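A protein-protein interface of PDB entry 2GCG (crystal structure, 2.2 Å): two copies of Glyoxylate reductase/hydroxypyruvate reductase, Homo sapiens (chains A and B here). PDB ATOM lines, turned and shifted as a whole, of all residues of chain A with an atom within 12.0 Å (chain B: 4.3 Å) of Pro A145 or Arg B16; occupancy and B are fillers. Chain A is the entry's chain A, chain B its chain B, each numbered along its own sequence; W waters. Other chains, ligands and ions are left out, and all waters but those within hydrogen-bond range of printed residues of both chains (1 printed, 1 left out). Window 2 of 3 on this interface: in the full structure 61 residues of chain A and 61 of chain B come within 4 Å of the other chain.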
ATOM      1  N   ARG A 126      -1.730   4.224  22.694  1.00  0.00           N
ATOM      2  CA  ARG A 126      -2.435   4.626  21.467  1.00  0.00           C
ATOM      3  C   ARG A 126      -1.545   4.698  20.208  1.00  0.00           C
ATOM      4  O   ARG A 126      -2.026   5.069  19.138  1.00  0.00           O
ATOM      5  CB  ARG A 126      -3.308   5.868  21.678  1.00  0.00           C
ATOM      6  CG  ARG A 126      -4.498   5.631  22.691  1.00  0.00           C
ATOM      7  CD  ARG A 126      -5.599   4.662  22.140  1.00  0.00           C
ATOM      8  NE  ARG A 126      -6.102   5.127  20.853  1.00  0.00           N
ATOM      9  CZ  ARG A 126      -7.082   6.008  20.708  1.00  0.00           C
ATOM     10  NH1 ARG A 126      -7.424   6.411  19.512  1.00  0.00           N
ATOM     11  NH2 ARG A 126      -7.728   6.476  21.753  1.00  0.00           N
ATOM     12  N   ARG A 127      -0.262   4.312  20.331  1.00  0.00           N
ATOM     13  CA  ARG A 127       0.588   3.963  19.168  1.00  0.00           C
ATOM     14  C   ARG A 127       1.019   5.196  18.360  1.00  0.00           C
ATOM     15  O   ARG A 127       1.326   5.114  17.156  1.00  0.00           O
ATOM     16  CB  ARG A 127      -0.124   2.938  18.248  1.00  0.00           C
ATOM     17  CG  ARG A 127      -0.343   1.555  18.864  1.00  0.00           C
ATOM     18  CD  ARG A 127      -1.109   0.587  17.945  1.00  0.00           C
ATOM     19  NE  ARG A 127      -0.306   0.140  16.808  1.00  0.00           N
ATOM     20  CZ  ARG A 127      -0.732  -0.674  15.852  1.00  0.00           C
ATOM     21  NH1 ARG A 127      -1.962  -1.126  15.863  1.00  0.00           N
ATOM     22  NH2 ARG A 127       0.072  -1.017  14.862  1.00  0.00           N
ATOM     23  N   GLY A 139       2.767   6.410   4.263  1.00  0.00           N
ATOM     24  CA  GLY A 139       1.960   5.241   4.568  1.00  0.00           C
ATOM     25  C   GLY A 139       0.492   5.596   4.669  1.00  0.00           C
ATOM     26  O   GLY A 139      -0.380   4.813   4.293  1.00  0.00           O
ATOM     27  N   TRP A 140       0.213   6.785   5.156  1.00  0.00           N
ATOM     28  CA  TRP A 140      -1.150   7.287   5.196  1.00  0.00           C
ATOM     29  C   TRP A 140      -1.757   7.496   3.804  1.00  0.00           C
ATOM     30  O   TRP A 140      -1.211   8.216   2.962  1.00  0.00           O
ATOM     31  CB  TRP A 140      -1.154   8.580   5.981  1.00  0.00           C
ATOM     32  CG  TRP A 140      -2.482   9.198   6.343  1.00  0.00           C
ATOM     33  CD1 TRP A 140      -3.752   8.628   6.311  1.00  0.00           C
ATOM     34  CD2 TRP A 140      -2.656  10.548   6.808  1.00  0.00           C
ATOM     35  NE1 TRP A 140      -4.694   9.558   6.740  1.00  0.00           N
ATOM     36  CE2 TRP A 140      -4.040  10.733   7.064  1.00  0.00           C
ATOM     37  CE3 TRP A 140      -1.766  11.597   7.069  1.00  0.00           C
ATOM     38  CZ2 TRP A 140      -4.545  11.937   7.552  1.00  0.00           C
ATOM     39  CZ3 TRP A 140      -2.291  12.831   7.569  1.00  0.00           C
ATOM     40  CH2 TRP A 140      -3.658  12.989   7.759  1.00  0.00           C
ATOM     41  N   THR A 141      -2.906   6.855   3.584  1.00  0.00           N
ATOM     42  CA  THR A 141      -3.641   7.030   2.349  1.00  0.00           C
ATOM     43  C   THR A 141      -5.097   7.446   2.625  1.00  0.00           C
ATOM     44  O   THR A 141      -5.728   8.009   1.732  1.00  0.00           O
ATOM     45  CB  THR A 141      -3.604   5.793   1.447  1.00  0.00           C
ATOM     46  OG1 THR A 141      -4.349   4.770   2.072  1.00  0.00           O
ATOM     47  CG2 THR A 141      -2.171   5.259   1.226  1.00  0.00           C
ATOM     48  N   SER A 142      -5.625   7.189   3.830  1.00  0.00           N
ATOM     49  CA  SER A 142      -6.999   7.629   4.142  1.00  0.00           C
ATOM     50  C   SER A 142      -7.351   7.397   5.604  1.00  0.00           C
ATOM     51  O   SER A 142      -6.539   6.875   6.360  1.00  0.00           O
ATOM     52  CB  SER A 142      -8.026   6.887   3.292  1.00  0.00           C
ATOM     53  OG  SER A 142      -9.359   7.356   3.524  1.00  0.00           O
ATOM     54  N   TRP A 143      -8.562   7.796   5.986  1.00  0.00           N
ATOM     55  CA  TRP A 143      -9.137   7.306   7.240  1.00  0.00           C
ATOM     56  C   TRP A 143      -9.384   5.836   6.969  1.00  0.00           C
ATOM     57  O   TRP A 143      -9.952   5.457   5.903  1.00  0.00           O
ATOM     58  CB  TRP A 143     -10.417   8.019   7.579  1.00  0.00           C
ATOM     59  CG  TRP A 143     -10.968   7.666   8.938  1.00  0.00           C
ATOM     60  CD1 TRP A 143     -10.738   8.305  10.125  1.00  0.00           C
ATOM     61  CD2 TRP A 143     -11.849   6.572   9.231  1.00  0.00           C
ATOM     62  NE1 TRP A 143     -11.460   7.686  11.147  1.00  0.00           N
ATOM     63  CE2 TRP A 143     -12.135   6.616  10.621  1.00  0.00           C
ATOM     64  CE3 TRP A 143     -12.418   5.552   8.448  1.00  0.00           C
ATOM     65  CZ2 TRP A 143     -12.982   5.692  11.243  1.00  0.00           C
ATOM     66  CZ3 TRP A 143     -13.259   4.636   9.059  1.00  0.00           C
ATOM     67  CH2 TRP A 143     -13.542   4.715  10.455  1.00  0.00           C
ATOM     68  N   LYS A 144      -8.925   4.989   7.888  1.00  0.00           N
ATOM     69  CA  LYS A 144      -9.084   3.546   7.693  1.00  0.00           C
ATOM     70  C   LYS A 144      -9.613   2.924   8.955  1.00  0.00           C
ATOM     71  O   LYS A 144      -9.085   3.184  10.031  1.00  0.00           O
ATOM     72  CB  LYS A 144      -7.751   2.898   7.303  1.00  0.00           C
ATOM     73  CG  LYS A 144      -7.342   3.122   5.853  1.00  0.00           C
ATOM     74  CD  LYS A 144      -6.111   2.307   5.565  1.00  0.00           C
ATOM     75  CE  LYS A 144      -5.465   2.677   4.236  1.00  0.00           C
ATOM     76  NZ  LYS A 144      -4.269   1.758   3.952  1.00  0.00           N
ATOM     77  N   PRO A 145     -10.641   2.072   8.830  1.00  0.00           N
ATOM     78  CA  PRO A 145     -11.337   1.630  10.053  1.00  0.00           C
ATOM     79  C   PRO A 145     -10.523   0.685  10.964  1.00  0.00           C
ATOM     80  O   PRO A 145     -10.717   0.743  12.185  1.00  0.00           O
ATOM     81  CB  PRO A 145     -12.601   0.956   9.521  1.00  0.00           C
ATOM     82  CG  PRO A 145     -12.197   0.447   8.152  1.00  0.00           C
ATOM     83  CD  PRO A 145     -11.217   1.470   7.607  1.00  0.00           C
ATOM     84  N   LEU A 146      -9.602  -0.114  10.415  1.00  0.00           N
ATOM     85  CA  LEU A 146      -8.881  -1.077  11.229  1.00  0.00           C
ATOM     86  C   LEU A 146      -7.385  -0.855  11.346  1.00  0.00           C
ATOM     87  O   LEU A 146      -6.642  -1.793  11.593  1.00  0.00           O
ATOM     88  CB  LEU A 146      -9.168  -2.506  10.751  1.00  0.00           C
ATOM     89  CG  LEU A 146     -10.518  -3.108  11.180  1.00  0.00           C
ATOM     90  CD1 LEU A 146     -10.539  -4.573  10.811  1.00  0.00           C
ATOM     91  CD2 LEU A 146     -10.829  -2.906  12.690  1.00  0.00           C
ATOM     92  N   TRP A 147      -6.970   0.393  11.219  1.00  0.00           N
ATOM     93  CA  TRP A 147      -5.583   0.772  11.041  1.00  0.00           C
ATOM     94  C   TRP A 147      -5.159   1.548  12.276  1.00  0.00           C
ATOM     95  O   TRP A 147      -5.904   2.451  12.772  1.00  0.00           O
ATOM     96  CB  TRP A 147      -5.526   1.657   9.835  1.00  0.00           C
ATOM     97  CG  TRP A 147      -4.195   2.107   9.376  1.00  0.00           C
ATOM     98  CD1 TRP A 147      -3.138   1.326   9.011  1.00  0.00           C
ATOM     99  CD2 TRP A 147      -3.801   3.456   9.133  1.00  0.00           C
ATOM    100  NE1 TRP A 147      -2.095   2.118   8.609  1.00  0.00           N
ATOM    101  CE2 TRP A 147      -2.483   3.427   8.661  1.00  0.00           C
ATOM    102  CE3 TRP A 147      -4.436   4.699   9.297  1.00  0.00           C
ATOM    103  CZ2 TRP A 147      -1.773   4.594   8.334  1.00  0.00           C
ATOM    104  CZ3 TRP A 147      -3.715   5.866   8.982  1.00  0.00           C
ATOM    105  CH2 TRP A 147      -2.401   5.797   8.508  1.00  0.00           C
ATOM    106  N   LEU A 148      -4.002   1.169  12.817  1.00  0.00           N
ATOM    107  CA  LEU A 148      -3.394   1.882  13.965  1.00  0.00           C
ATOM    108  C   LEU A 148      -4.262   1.851  15.228  1.00  0.00           C
ATOM    109  O   LEU A 148      -4.241   2.767  16.103  1.00  0.00           O
ATOM    110  CB  LEU A 148      -3.013   3.298  13.569  1.00  0.00           C
ATOM    111  CG  LEU A 148      -1.685   3.391  12.802  1.00  0.00           C
ATOM    112  CD1 LEU A 148      -1.692   4.609  11.878  1.00  0.00           C
ATOM    113  CD2 LEU A 148      -0.481   3.457  13.749  1.00  0.00           C
ATOM    114  N   CYS A 149      -5.056   0.790  15.309  1.00  0.00           N
ATOM    115  CA  CYS A 149      -5.873   0.571  16.480  1.00  0.00           C
ATOM    116  C   CYS A 149      -4.988   0.227  17.698  1.00  0.00           C
ATOM    117  O   CYS A 149      -4.088  -0.630  17.635  1.00  0.00           O
ATOM    118  CB  CYS A 149      -6.959  -0.469  16.185  1.00  0.00           C
ATOM    119  SG  CYS A 149      -8.281   0.167  15.143  1.00  0.00           S
ATOM    120  N   GLY A 150      -5.220   0.959  18.777  1.00  0.00           N
ATOM    121  CA  GLY A 150      -4.486   0.841  20.029  1.00  0.00           C
ATOM    122  C   GLY A 150      -5.314   0.262  21.175  1.00  0.00           C
ATOM    123  O   GLY A 150      -6.418  -0.305  20.968  1.00  0.00           O
ATOM    124  N   TYR A 151      -4.782   0.399  22.380  1.00  0.00           N
ATOM    125  CA  TYR A 151      -5.376  -0.256  23.584  1.00  0.00           C
ATOM    126  C   TYR A 151      -5.918   0.795  24.485  1.00  0.00           C
ATOM    127  O   TYR A 151      -5.147   1.669  24.965  1.00  0.00           O
ATOM    128  CB  TYR A 151      -4.313  -1.082  24.345  1.00  0.00           C
ATOM    129  CG  TYR A 151      -3.525  -1.944  23.394  1.00  0.00           C
ATOM    130  CD1 TYR A 151      -4.015  -3.192  23.008  1.00  0.00           C
ATOM    131  CD2 TYR A 151      -2.339  -1.471  22.801  1.00  0.00           C
ATOM    132  CE1 TYR A 151      -3.332  -3.987  22.103  1.00  0.00           C
ATOM    133  CE2 TYR A 151      -1.627  -2.271  21.877  1.00  0.00           C
ATOM    134  CZ  TYR A 151      -2.142  -3.526  21.535  1.00  0.00           C
ATOM    135  OH  TYR A 151      -1.504  -4.334  20.617  1.00  0.00           O
ATOM    136  N   ARG B  15     -16.050   0.311   1.559  1.00  0.00           N
ATOM    137  CA  ARG B  15     -14.754  -0.136   2.117  1.00  0.00           C
ATOM    138  C   ARG B  15     -14.931  -1.468   2.826  1.00  0.00           C
ATOM    139  O   ARG B  15     -16.075  -1.843   3.143  1.00  0.00           O
ATOM    140  CB  ARG B  15     -14.201   0.898   3.144  1.00  0.00           C
ATOM    141  CG  ARG B  15     -12.692   0.902   3.351  1.00  0.00           C
ATOM    142  CD  ARG B  15     -11.933   1.675   2.258  1.00  0.00           C
ATOM    143  NE  ARG B  15     -12.150   3.131   2.295  1.00  0.00           N
ATOM    144  CZ  ARG B  15     -11.519   3.980   3.112  1.00  0.00           C
ATOM    145  NH1 ARG B  15     -10.643   3.543   3.982  1.00  0.00           N
ATOM    146  NH2 ARG B  15     -11.761   5.282   3.053  1.00  0.00           N
ATOM    147  N   ARG B  16     -13.812  -2.174   3.086  1.00  0.00           N
ATOM    148  CA  ARG B  16     -13.831  -3.247   4.096  1.00  0.00           C
ATOM    149  C   ARG B  16     -14.124  -2.679   5.466  1.00  0.00           C
ATOM    150  O   ARG B  16     -13.276  -1.998   6.049  1.00  0.00           O
ATOM    151  CB  ARG B  16     -12.523  -4.036   4.171  1.00  0.00           C
ATOM    152  CG  ARG B  16     -12.578  -5.237   5.110  1.00  0.00           C
ATOM    153  CD  ARG B  16     -11.791  -6.419   4.549  1.00  0.00           C
ATOM    154  NE  ARG B  16     -10.593  -5.892   3.935  1.00  0.00           N
ATOM    155  CZ  ARG B  16     -10.014  -6.339   2.833  1.00  0.00           C
ATOM    156  NH1 ARG B  16     -10.486  -7.403   2.172  1.00  0.00           N
ATOM    157  NH2 ARG B  16      -8.934  -5.696   2.408  1.00  0.00           N
ATOM    158  N   ILE B  17     -15.298  -2.991   6.003  1.00  0.00           N
ATOM    159  CA  ILE B  17     -15.547  -2.611   7.382  1.00  0.00           C
ATOM    160  C   ILE B  17     -15.187  -3.731   8.368  1.00  0.00           C
ATOM    161  O   ILE B  17     -15.095  -4.885   7.966  1.00  0.00           O
ATOM    162  CB  ILE B  17     -16.977  -1.988   7.608  1.00  0.00           C
ATOM    163  CG1 ILE B  17     -18.096  -2.976   7.270  1.00  0.00           C
ATOM    164  CG2 ILE B  17     -17.088  -0.615   6.877  1.00  0.00           C
ATOM    165  CD1 ILE B  17     -19.474  -2.440   7.635  1.00  0.00           C
ATOM    166  N   PRO B  18     -14.876  -3.378   9.633  1.00  0.00           N
ATOM    167  CA  PRO B  18     -14.703  -4.378  10.661  1.00  0.00           C
ATOM    168  C   PRO B  18     -15.823  -5.434  10.634  1.00  0.00           C
ATOM    169  O   PRO B  18     -17.011  -5.085  10.528  1.00  0.00           O
ATOM    170  CB  PRO B  18     -14.799  -3.561  11.938  1.00  0.00           C
ATOM    171  CG  PRO B  18     -14.251  -2.249  11.586  1.00  0.00           C
ATOM    172  CD  PRO B  18     -14.614  -2.020  10.154  1.00  0.00           C
ATOM    173  N   ARG B  22     -20.053  -6.259   9.013  1.00  0.00           N
ATOM    174  CA  ARG B  22     -20.048  -6.952   7.726  1.00  0.00           C
ATOM    175  C   ARG B  22     -20.851  -8.230   7.868  1.00  0.00           C
ATOM    176  O   ARG B  22     -21.564  -8.665   6.952  1.00  0.00           O
ATOM    177  CB  ARG B  22     -18.600  -7.317   7.429  1.00  0.00           C
ATOM    178  CG  ARG B  22     -18.070  -6.967   6.059  1.00  0.00           C
ATOM    179  CD  ARG B  22     -16.523  -6.880   6.062  1.00  0.00           C
ATOM    180  NE  ARG B  22     -15.909  -8.158   6.382  1.00  0.00           N
ATOM    181  CZ  ARG B  22     -14.786  -8.318   7.070  1.00  0.00           C
ATOM    182  NH1 ARG B  22     -14.127  -7.277   7.527  1.00  0.00           N
ATOM    183  NH2 ARG B  22     -14.316  -9.538   7.304  1.00  0.00           N
ATOM    184  N   TRP B  36     -16.935  -2.460  -1.844  1.00  0.00           N
ATOM    185  CA  TRP B  36     -15.625  -2.072  -2.346  1.00  0.00           C
ATOM    186  C   TRP B  36     -14.709  -2.925  -1.476  1.00  0.00           C
ATOM    187  O   TRP B  36     -14.614  -2.699  -0.259  1.00  0.00           O
ATOM    188  CB  TRP B  36     -15.397  -0.585  -2.088  1.00  0.00           C
ATOM    189  CG  TRP B  36     -14.064  -0.037  -2.466  1.00  0.00           C
ATOM    190  CD1 TRP B  36     -13.119   0.481  -1.617  1.00  0.00           C
ATOM    191  CD2 TRP B  36     -13.532   0.097  -3.790  1.00  0.00           C
ATOM    192  NE1 TRP B  36     -12.029   0.924  -2.332  1.00  0.00           N
ATOM    193  CE2 TRP B  36     -12.258   0.713  -3.669  1.00  0.00           C
ATOM    194  CE3 TRP B  36     -14.003  -0.243  -5.075  1.00  0.00           C
ATOM    195  CZ2 TRP B  36     -11.428   0.963  -4.788  1.00  0.00           C
ATOM    196  CZ3 TRP B  36     -13.186   0.034  -6.188  1.00  0.00           C
ATOM    197  CH2 TRP B  36     -11.922   0.643  -6.031  1.00  0.00           C
ATOM    198  N   SER B  38     -11.710  -3.663  -0.223  1.00  0.00           N
ATOM    199  CA  SER B  38     -10.413  -2.997  -0.152  1.00  0.00           C
ATOM    200  C   SER B  38     -10.279  -2.169   1.110  1.00  0.00           C
ATOM    201  O   SER B  38     -11.272  -1.733   1.688  1.00  0.00           O
ATOM    202  CB  SER B  38     -10.248  -2.071  -1.390  1.00  0.00           C
ATOM    203  OG  SER B  38      -9.108  -1.222  -1.281  1.00  0.00           O
ATOM    204  N   ASP B  39      -9.041  -1.921   1.510  1.00  0.00           N
ATOM    205  CA  ASP B  39      -8.759  -1.015   2.605  1.00  0.00           C
ATOM    206  C   ASP B  39      -8.482   0.387   2.130  1.00  0.00           C
ATOM    207  O   ASP B  39      -8.320   1.306   2.946  1.00  0.00           O
ATOM    208  CB  ASP B  39      -7.558  -1.534   3.399  1.00  0.00           C
ATOM    209  CG  ASP B  39      -7.840  -2.859   4.053  1.00  0.00           C
ATOM    210  OD1 ASP B  39      -6.896  -3.656   4.104  1.00  0.00           O
ATOM    211  OD2 ASP B  39      -9.019  -3.127   4.464  1.00  0.00           O
ATOM    212  N   MET B  83     -20.139   5.614   9.003  1.00  0.00           N
ATOM    213  CA  MET B  83     -19.417   5.047  10.089  1.00  0.00           C
ATOM    214  C   MET B  83     -18.567   6.155  10.738  1.00  0.00           C
ATOM    215  O   MET B  83     -17.317   6.152  10.653  1.00  0.00           O
ATOM    216  CB  MET B  83     -18.559   3.883   9.573  1.00  0.00           C
ATOM    217  CG  MET B  83     -18.155   2.878  10.661  1.00  0.00           C
ATOM    218  SD  MET B  83     -16.972   1.618  10.111  1.00  0.00           S
ATOM    219  CE  MET B  83     -15.914   1.423  11.574  1.00  0.00           C
ATOM    220  N   ARG B 304     -13.988   0.438  17.250  1.00  0.00           N
ATOM    221  CA  ARG B 304     -14.174   0.445  15.800  1.00  0.00           C
ATOM    222  C   ARG B 304     -15.187  -0.617  15.419  1.00  0.00           C
ATOM    223  O   ARG B 304     -16.055  -0.333  14.597  1.00  0.00           O
ATOM    224  CB  ARG B 304     -12.837   0.331  15.002  1.00  0.00           C
ATOM    225  CG  ARG B 304     -12.027   1.610  15.021  1.00  0.00           C
ATOM    226  CD  ARG B 304     -12.564   2.668  14.011  1.00  0.00           C
ATOM    227  NE  ARG B 304     -11.914   3.971  14.136  1.00  0.00           N
ATOM    228  CZ  ARG B 304     -10.715   4.256  13.609  1.00  0.00           C
ATOM    229  NH1 ARG B 304     -10.073   3.332  12.884  1.00  0.00           N
ATOM    230  NH2 ARG B 304     -10.185   5.469  13.778  1.00  0.00           N
HETATM  231  O   HOH W   1      -7.745   5.044  12.316  1.00  0.00           O
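The backbone carbonyl oxygen (O) of Ser A142 lies within hydrogen-bond range of the indole nitrogen (NE1) of Trp A140 (3.3 Å).
The backbone carbonyl oxygen of Asp B39 lies within hydrogen-bond range of the guanidinium group of Arg B15, at 3.4 Å.
The backbone NH (N) of Arg B16 is in hydrogen-bond range of the backbone carbonyl oxygen (O) of Trp B36 (3.5 Å).
The backbone carbonyl oxygen (O) of Ser B38 sits at hydrogen-bond distance from the backbone NH (N) of Arg B16 (2.9 Å).
NE of Arg B16 is in salt-bridge range of OD2 of Asp B39 (3.2 Å).
Trp A143 touches Arg B304.
Arg B15 touches Lys A144.
O of Asp B39 touches CE of Lys A144, at 3.4 Å.
Arg B16 touches Pro A145 (O to CG, 3.4 Å).
CB of Pro A145 touches CD of Pro B18, 3.6 Å away.
Pro A145 touches Met B83.
Leu A146 touches Pro B18 (CD2 to CG, 3.7 Å).
The side-chain hydroxyl (OG) of Ser A142 lies within hydrogen-bond range of the guanidinium group (NH2) of Arg B15 (3.2 Å).
The backbone carbonyl oxygen of Trp A143 lies within hydrogen-bond range of the guanidinium group of Arg B15 (2.8 Å).
O of Lys A144 lies within hydrogen-bond range of NH1 of Arg B304, at 3.0 Å.
O of Pro A145 is in hydrogen-bond range of NH1 of Arg B304 (2.8 Å).
Hydrophobic or aromatic side chains of chain A that line the printed part of chain B: Trp A143, Pro A145 and Leu A146.
Of the 10 printed residues of chain B, 6 touch a printed residue of chain A.
Among the printed residues, 11 pairs touch across the chains.
Among the printed residues, no Asp or Glu carboxylate lies within 4 Å of a Lys or Arg side-chain nitrogen of the other chain.
Water W1 lies within hydrogen-bond range of NH2 of Arg B304 (2.9 Å), O of Trp A147 (3.2 Å) and O of Lys A144 (3.2 Å).
Pro A145 touches four residues of chain B.
Arg B16 touches just one residue of chain A: Pro A145 (3.4 Å).
Arg B15 touches three residues of chain A.
No residue of chain A comes within 4 Å of Ile B17.
Of chain A, only Pro A145 (3.6 Å) and Leu A146 (3.7 Å) come within 4 Å of Pro B18.
No residue of chain A comes within 4 Å of Ser B38.
Printed residues of chain B within 4 Å of Lys A144: Arg B15 (3.8 Å), Asp B39 (3.4 Å) and Arg B304 (3.0 Å).
Of the printed residues of chain B, Trp A143 touches Arg B15 (2.8 Å) and Arg B304 (3.5 Å).
Printed residues of chain A within 4 Å of Arg B304: Trp A143, Lys A144 and Pro A145.
Printed residues of chain B within 4 Å of Ser A142: Arg B15.
Of the printed residues of chain A, Met B83 touches Pro A145 (3.9 Å).
The nearest residue of chain B that does not touch Pro A145 is Arg B15 (4.2 Å).
The nearest printed residue of chain B that does not touch Ser A142 is Asp B39 (5.6 Å).
No position is printed for both chains.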
